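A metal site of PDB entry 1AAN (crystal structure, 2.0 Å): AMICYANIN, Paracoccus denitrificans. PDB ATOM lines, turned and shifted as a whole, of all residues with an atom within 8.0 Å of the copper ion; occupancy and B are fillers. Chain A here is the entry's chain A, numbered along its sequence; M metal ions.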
ATOM      1  N   ILE A  25     -26.183  20.349   0.420  1.00  0.00           N
ATOM      2  CA  ILE A  25     -25.909  21.746   0.729  1.00  0.00           C
ATOM      3  C   ILE A  25     -27.093  22.107   1.623  1.00  0.00           C
ATOM      4  O   ILE A  25     -28.228  21.895   1.199  1.00  0.00           O
ATOM      5  CB  ILE A  25     -25.917  22.590  -0.560  1.00  0.00           C
ATOM      6  CG1 ILE A  25     -24.902  22.070  -1.567  1.00  0.00           C
ATOM      7  CG2 ILE A  25     -25.614  24.044  -0.171  1.00  0.00           C
ATOM      8  CD1 ILE A  25     -25.037  22.748  -2.937  1.00  0.00           C
ATOM      9  N   MET A  28     -26.642  27.146   4.435  1.00  0.00           N
ATOM     10  CA  MET A  28     -25.594  27.939   3.785  1.00  0.00           C
ATOM     11  C   MET A  28     -24.208  27.329   3.906  1.00  0.00           C
ATOM     12  O   MET A  28     -23.210  28.051   4.045  1.00  0.00           O
ATOM     13  CB  MET A  28     -25.546  29.362   4.375  1.00  0.00           C
ATOM     14  CG  MET A  28     -26.831  30.154   4.271  1.00  0.00           C
ATOM     15  SD  MET A  28     -27.436  30.451   2.580  1.00  0.00           S
ATOM     16  CE  MET A  28     -26.207  31.611   2.063  1.00  0.00           C
ATOM     17  N   LYS A  29     -24.107  25.982   3.856  1.00  0.00           N
ATOM     18  CA  LYS A  29     -22.849  25.246   3.993  1.00  0.00           C
ATOM     19  C   LYS A  29     -22.864  24.043   3.087  1.00  0.00           C
ATOM     20  O   LYS A  29     -23.930  23.509   2.768  1.00  0.00           O
ATOM     21  CB  LYS A  29     -22.626  24.679   5.399  1.00  0.00           C
ATOM     22  CG  LYS A  29     -22.477  25.716   6.473  1.00  0.00           C
ATOM     23  CD  LYS A  29     -22.584  25.135   7.870  1.00  0.00           C
ATOM     24  CE  LYS A  29     -22.547  26.386   8.729  1.00  0.00           C
ATOM     25  NZ  LYS A  29     -22.736  26.048  10.114  1.00  0.00           N
ATOM     26  N   TYR A  30     -21.677  23.598   2.639  1.00  0.00           N
ATOM     27  CA  TYR A  30     -21.578  22.322   1.952  1.00  0.00           C
ATOM     28  C   TYR A  30     -21.392  21.347   3.113  1.00  0.00           C
ATOM     29  O   TYR A  30     -20.412  21.477   3.864  1.00  0.00           O
ATOM     30  CB  TYR A  30     -20.336  22.287   1.053  1.00  0.00           C
ATOM     31  CG  TYR A  30     -20.383  23.298  -0.097  1.00  0.00           C
ATOM     32  CD1 TYR A  30     -21.231  23.065  -1.168  1.00  0.00           C
ATOM     33  CD2 TYR A  30     -19.561  24.418  -0.069  1.00  0.00           C
ATOM     34  CE1 TYR A  30     -21.252  23.964  -2.212  1.00  0.00           C
ATOM     35  CE2 TYR A  30     -19.581  25.317  -1.113  1.00  0.00           C
ATOM     36  CZ  TYR A  30     -20.421  25.079  -2.184  1.00  0.00           C
ATOM     37  OH  TYR A  30     -20.436  25.966  -3.248  1.00  0.00           O
ATOM     38  N   ASN A  47     -28.864  20.525  -3.515  1.00  0.00           N
ATOM     39  CA  ASN A  47     -29.285  21.659  -2.721  1.00  0.00           C
ATOM     40  C   ASN A  47     -30.558  21.293  -1.969  1.00  0.00           C
ATOM     41  O   ASN A  47     -31.592  20.976  -2.568  1.00  0.00           O
ATOM     42  CB  ASN A  47     -29.572  22.871  -3.581  1.00  0.00           C
ATOM     43  CG  ASN A  47     -29.782  24.119  -2.757  1.00  0.00           C
ATOM     44  OD1 ASN A  47     -30.099  25.163  -3.312  1.00  0.00           O
ATOM     45  ND2 ASN A  47     -29.596  24.191  -1.452  1.00  0.00           N
ATOM     46  N   GLU A  49     -31.959  23.365   0.319  1.00  0.00           N
ATOM     47  CA  GLU A  49     -32.641  24.500   0.880  1.00  0.00           C
ATOM     48  C   GLU A  49     -33.125  25.430  -0.197  1.00  0.00           C
ATOM     49  O   GLU A  49     -32.687  25.286  -1.340  1.00  0.00           O
ATOM     50  CB  GLU A  49     -31.724  25.224   1.826  1.00  0.00           C
ATOM     51  CG  GLU A  49     -30.445  25.866   1.337  1.00  0.00           C
ATOM     52  CD  GLU A  49     -29.711  26.593   2.456  1.00  0.00           C
ATOM     53  OE1 GLU A  49     -30.236  26.745   3.562  1.00  0.00           O
ATOM     54  OE2 GLU A  49     -28.594  27.026   2.248  1.00  0.00           O
ATOM     55  N   MET A  51     -32.707  28.698  -0.748  1.00  0.00           N
ATOM     56  CA  MET A  51     -31.717  29.641  -1.278  1.00  0.00           C
ATOM     57  C   MET A  51     -30.899  28.925  -2.359  1.00  0.00           C
ATOM     58  O   MET A  51     -30.334  27.896  -2.033  1.00  0.00           O
ATOM     59  CB  MET A  51     -30.779  30.103  -0.172  1.00  0.00           C
ATOM     60  CG  MET A  51     -29.716  31.140  -0.514  1.00  0.00           C
ATOM     61  SD  MET A  51     -30.346  32.650  -1.304  1.00  0.00           S
ATOM     62  CE  MET A  51     -31.317  33.433  -0.056  1.00  0.00           C
ATOM     63  N   PRO A  52     -30.849  29.383  -3.610  1.00  0.00           N
ATOM     64  CA  PRO A  52     -30.099  28.755  -4.687  1.00  0.00           C
ATOM     65  C   PRO A  52     -28.595  28.749  -4.417  1.00  0.00           C
ATOM     66  O   PRO A  52     -28.023  29.722  -3.910  1.00  0.00           O
ATOM     67  CB  PRO A  52     -30.464  29.548  -5.930  1.00  0.00           C
ATOM     68  CG  PRO A  52     -31.853  30.038  -5.609  1.00  0.00           C
ATOM     69  CD  PRO A  52     -31.648  30.487  -4.155  1.00  0.00           C
ATOM     70  N   HIS A  53     -27.906  27.664  -4.769  1.00  0.00           N
ATOM     71  CA  HIS A  53     -26.466  27.601  -4.591  1.00  0.00           C
ATOM     72  C   HIS A  53     -25.857  26.940  -5.806  1.00  0.00           C
ATOM     73  O   HIS A  53     -26.560  26.305  -6.572  1.00  0.00           O
ATOM     74  CB  HIS A  53     -26.084  26.750  -3.372  1.00  0.00           C
ATOM     75  CG  HIS A  53     -26.566  27.276  -2.019  1.00  0.00           C
ATOM     76  ND1 HIS A  53     -26.004  28.316  -1.438  1.00  0.00           N
ATOM     77  CD2 HIS A  53     -27.558  26.710  -1.268  1.00  0.00           C
ATOM     78  CE1 HIS A  53     -26.642  28.438  -0.303  1.00  0.00           C
ATOM     79  NE2 HIS A  53     -27.552  27.499  -0.211  1.00  0.00           N
ATOM     80  N   ASN A  54     -24.558  27.062  -6.046  1.00  0.00           N
ATOM     81  CA  ASN A  54     -23.925  26.331  -7.137  1.00  0.00           C
ATOM     82  C   ASN A  54     -22.541  25.928  -6.612  1.00  0.00           C
ATOM     83  O   ASN A  54     -22.263  26.103  -5.419  1.00  0.00           O
ATOM     84  CB  ASN A  54     -23.783  27.252  -8.369  1.00  0.00           C
ATOM     85  CG  ASN A  54     -22.730  28.363  -8.254  1.00  0.00           C
ATOM     86  OD1 ASN A  54     -22.379  28.830  -7.165  1.00  0.00           O
ATOM     87  ND2 ASN A  54     -22.202  28.839  -9.377  1.00  0.00           N
ATOM     88  N   VAL A  55     -21.687  25.344  -7.463  1.00  0.00           N
ATOM     89  CA  VAL A  55     -20.287  25.124  -7.158  1.00  0.00           C
ATOM     90  C   VAL A  55     -19.543  25.860  -8.270  1.00  0.00           C
ATOM     91  O   VAL A  55     -19.941  25.849  -9.432  1.00  0.00           O
ATOM     92  CB  VAL A  55     -19.913  23.603  -7.155  1.00  0.00           C
ATOM     93  CG1 VAL A  55     -20.680  23.001  -6.002  1.00  0.00           C
ATOM     94  CG2 VAL A  55     -20.290  22.838  -8.427  1.00  0.00           C
ATOM     95  N   MET A  71     -27.054  27.489 -11.146  1.00  0.00           N
ATOM     96  CA  MET A  71     -27.670  27.649  -9.844  1.00  0.00           C
ATOM     97  C   MET A  71     -28.699  26.527  -9.633  1.00  0.00           C
ATOM     98  O   MET A  71     -29.508  26.206 -10.522  1.00  0.00           O
ATOM     99  CB  MET A  71     -28.343  29.007  -9.762  1.00  0.00           C
ATOM    100  CG  MET A  71     -27.416  30.214  -9.931  1.00  0.00           C
ATOM    101  SD  MET A  71     -25.953  30.270  -8.847  1.00  0.00           S
ATOM    102  CE  MET A  71     -26.774  30.319  -7.284  1.00  0.00           C
ATOM    103  N   MET A  72     -28.600  25.853  -8.482  1.00  0.00           N
ATOM    104  CA  MET A  72     -29.473  24.748  -8.139  1.00  0.00           C
ATOM    105  C   MET A  72     -30.516  25.306  -7.204  1.00  0.00           C
ATOM    106  O   MET A  72     -30.184  25.992  -6.229  1.00  0.00           O
ATOM    107  CB  MET A  72     -28.724  23.648  -7.399  1.00  0.00           C
ATOM    108  CG  MET A  72     -27.745  22.862  -8.244  1.00  0.00           C
ATOM    109  SD  MET A  72     -26.694  21.820  -7.199  1.00  0.00           S
ATOM    110  CE  MET A  72     -25.446  22.975  -6.814  1.00  0.00           C
ATOM    111  N   HIS A  91     -16.161  27.137  -4.551  1.00  0.00           N
ATOM    112  CA  HIS A  91     -16.948  27.974  -3.693  1.00  0.00           C
ATOM    113  C   HIS A  91     -18.313  28.168  -4.318  1.00  0.00           C
ATOM    114  O   HIS A  91     -18.563  27.681  -5.426  1.00  0.00           O
ATOM    115  CB  HIS A  91     -16.210  29.302  -3.483  1.00  0.00           C
ATOM    116  CG  HIS A  91     -16.057  30.178  -4.706  1.00  0.00           C
ATOM    117  ND1 HIS A  91     -15.146  30.059  -5.666  1.00  0.00           N
ATOM    118  CD2 HIS A  91     -16.848  31.263  -5.002  1.00  0.00           C
ATOM    119  CE1 HIS A  91     -15.337  31.011  -6.533  1.00  0.00           C
ATOM    120  NE2 HIS A  91     -16.356  31.733  -6.129  1.00  0.00           N
ATOM    121  N   CYS A  92     -19.196  28.883  -3.637  1.00  0.00           N
ATOM    122  CA  CYS A  92     -20.503  29.193  -4.181  1.00  0.00           C
ATOM    123  C   CYS A  92     -20.410  30.602  -4.771  1.00  0.00           C
ATOM    124  O   CYS A  92     -20.017  31.540  -4.066  1.00  0.00           O
ATOM    125  CB  CYS A  92     -21.539  29.159  -3.054  1.00  0.00           C
ATOM    126  SG  CYS A  92     -23.199  29.503  -3.694  1.00  0.00           S
ATOM    127  N   THR A  93     -20.698  30.824  -6.071  1.00  0.00           N
ATOM    128  CA  THR A  93     -20.610  32.156  -6.683  1.00  0.00           C
ATOM    129  C   THR A  93     -21.346  33.261  -5.890  1.00  0.00           C
ATOM    130  O   THR A  93     -20.658  34.227  -5.517  1.00  0.00           O
ATOM    131  CB  THR A  93     -21.158  32.078  -8.130  1.00  0.00           C
ATOM    132  OG1 THR A  93     -20.447  31.031  -8.784  1.00  0.00           O
ATOM    133  CG2 THR A  93     -20.978  33.379  -8.917  1.00  0.00           C
ATOM    134  N   PRO A  94     -22.655  33.251  -5.531  1.00  0.00           N
ATOM    135  CA  PRO A  94     -23.261  34.351  -4.787  1.00  0.00           C
ATOM    136  C   PRO A  94     -22.872  34.443  -3.332  1.00  0.00           C
ATOM    137  O   PRO A  94     -23.105  35.470  -2.697  1.00  0.00           O
ATOM    138  CB  PRO A  94     -24.742  34.148  -4.986  1.00  0.00           C
ATOM    139  CG  PRO A  94     -24.853  32.641  -5.062  1.00  0.00           C
ATOM    140  CD  PRO A  94     -23.658  32.255  -5.905  1.00  0.00           C
ATOM    141  N   HIS A  95     -22.301  33.329  -2.808  1.00  0.00           N
ATOM    142  CA  HIS A  95     -22.017  33.208  -1.381  1.00  0.00           C
ATOM    143  C   HIS A  95     -20.570  32.746  -1.218  1.00  0.00           C
ATOM    144  O   HIS A  95     -20.370  31.604  -0.792  1.00  0.00           O
ATOM    145  CB  HIS A  95     -22.965  32.186  -0.728  1.00  0.00           C
ATOM    146  CG  HIS A  95     -24.452  32.367  -1.053  1.00  0.00           C
ATOM    147  ND1 HIS A  95     -25.114  31.397  -1.655  1.00  0.00           N
ATOM    148  CD2 HIS A  95     -25.210  33.472  -0.763  1.00  0.00           C
ATOM    149  CE1 HIS A  95     -26.331  31.872  -1.755  1.00  0.00           C
ATOM    150  NE2 HIS A  95     -26.395  33.091  -1.229  1.00  0.00           N
ATOM    151  N   PRO A  96     -19.521  33.524  -1.540  1.00  0.00           N
ATOM    152  CA  PRO A  96     -18.131  33.069  -1.587  1.00  0.00           C
ATOM    153  C   PRO A  96     -17.597  32.573  -0.254  1.00  0.00           C
ATOM    154  O   PRO A  96     -16.568  31.919  -0.173  1.00  0.00           O
ATOM    155  CB  PRO A  96     -17.334  34.252  -2.066  1.00  0.00           C
ATOM    156  CG  PRO A  96     -18.328  35.271  -2.509  1.00  0.00           C
ATOM    157  CD  PRO A  96     -19.601  34.951  -1.774  1.00  0.00           C
ATOM    158  N   PHE A  97     -18.239  32.917   0.866  1.00  0.00           N
ATOM    159  CA  PHE A  97     -17.817  32.377   2.166  1.00  0.00           C
ATOM    160  C   PHE A  97     -18.134  30.873   2.229  1.00  0.00           C
ATOM    161  O   PHE A  97     -17.636  30.186   3.117  1.00  0.00           O
ATOM    162  CB  PHE A  97     -18.522  33.163   3.300  1.00  0.00           C
ATOM    163  CG  PHE A  97     -20.043  33.244   3.147  1.00  0.00           C
ATOM    164  CD1 PHE A  97     -20.843  32.174   3.490  1.00  0.00           C
ATOM    165  CD2 PHE A  97     -20.609  34.393   2.599  1.00  0.00           C
ATOM    166  CE1 PHE A  97     -22.210  32.230   3.281  1.00  0.00           C
ATOM    167  CE2 PHE A  97     -21.970  34.438   2.397  1.00  0.00           C
ATOM    168  CZ  PHE A  97     -22.774  33.362   2.734  1.00  0.00           C
ATOM    169  N   MET A  98     -18.955  30.298   1.338  1.00  0.00           N
ATOM    170  CA  MET A  98     -19.212  28.855   1.287  1.00  0.00           C
ATOM    171  C   MET A  98     -18.095  28.286   0.433  1.00  0.00           C
ATOM    172  O   MET A  98     -18.012  28.601  -0.745  1.00  0.00           O
ATOM    173  CB  MET A  98     -20.526  28.515   0.599  1.00  0.00           C
ATOM    174  CG  MET A  98     -21.758  28.991   1.302  1.00  0.00           C
ATOM    175  SD  MET A  98     -23.249  28.621   0.335  1.00  0.00           S
ATOM    176  CE  MET A  98     -23.283  26.857   0.273  1.00  0.00           C
HETATM  177 CU    CU M   1     -24.593  29.512  -2.060  1.00  0.00          CU
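The side-chain sulfur of Met 98 sits close to a ring nitrogen (ND1) of His 53, at 3.3 Å. NE2 of His 53 sits close to O of Met 51. A ring nitrogen (NE2) of His 53 sits at hydrogen-bond distance from the side-chain carboxylate (OE2) of Glu 49 (2.7 Å). N of Met 72 sits at hydrogen-bond distance from O of His 53, at 2.8 Å. O of Met 98 is in hydrogen-bond range of N of Cys 92, 3.1 Å away. The side-chain sulfur (SG) of Cys 92 sits close to the side-chain amide oxygen (OD1) of Asn 54, at 3.6 Å. The side-chain hydroxyl (OH) of Tyr 30 sits at hydrogen-bond distance from the backbone NH (N) of Cys 92, 3.2 Å away.
Merely in contact with the copper ion: Pro 52. The nearest printed residue that does not touch the copper ion is Pro 94 (4.3 Å).
ND1 of His 53 binds the copper ion (2.0 Å). The copper ion is bound by a ring nitrogen (ND1) of His 95 (2.0 Å). The copper ion is bound by SG of Cys 92. Slightly farther from the copper ion lies SD of Met 98 (2.9 Å).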
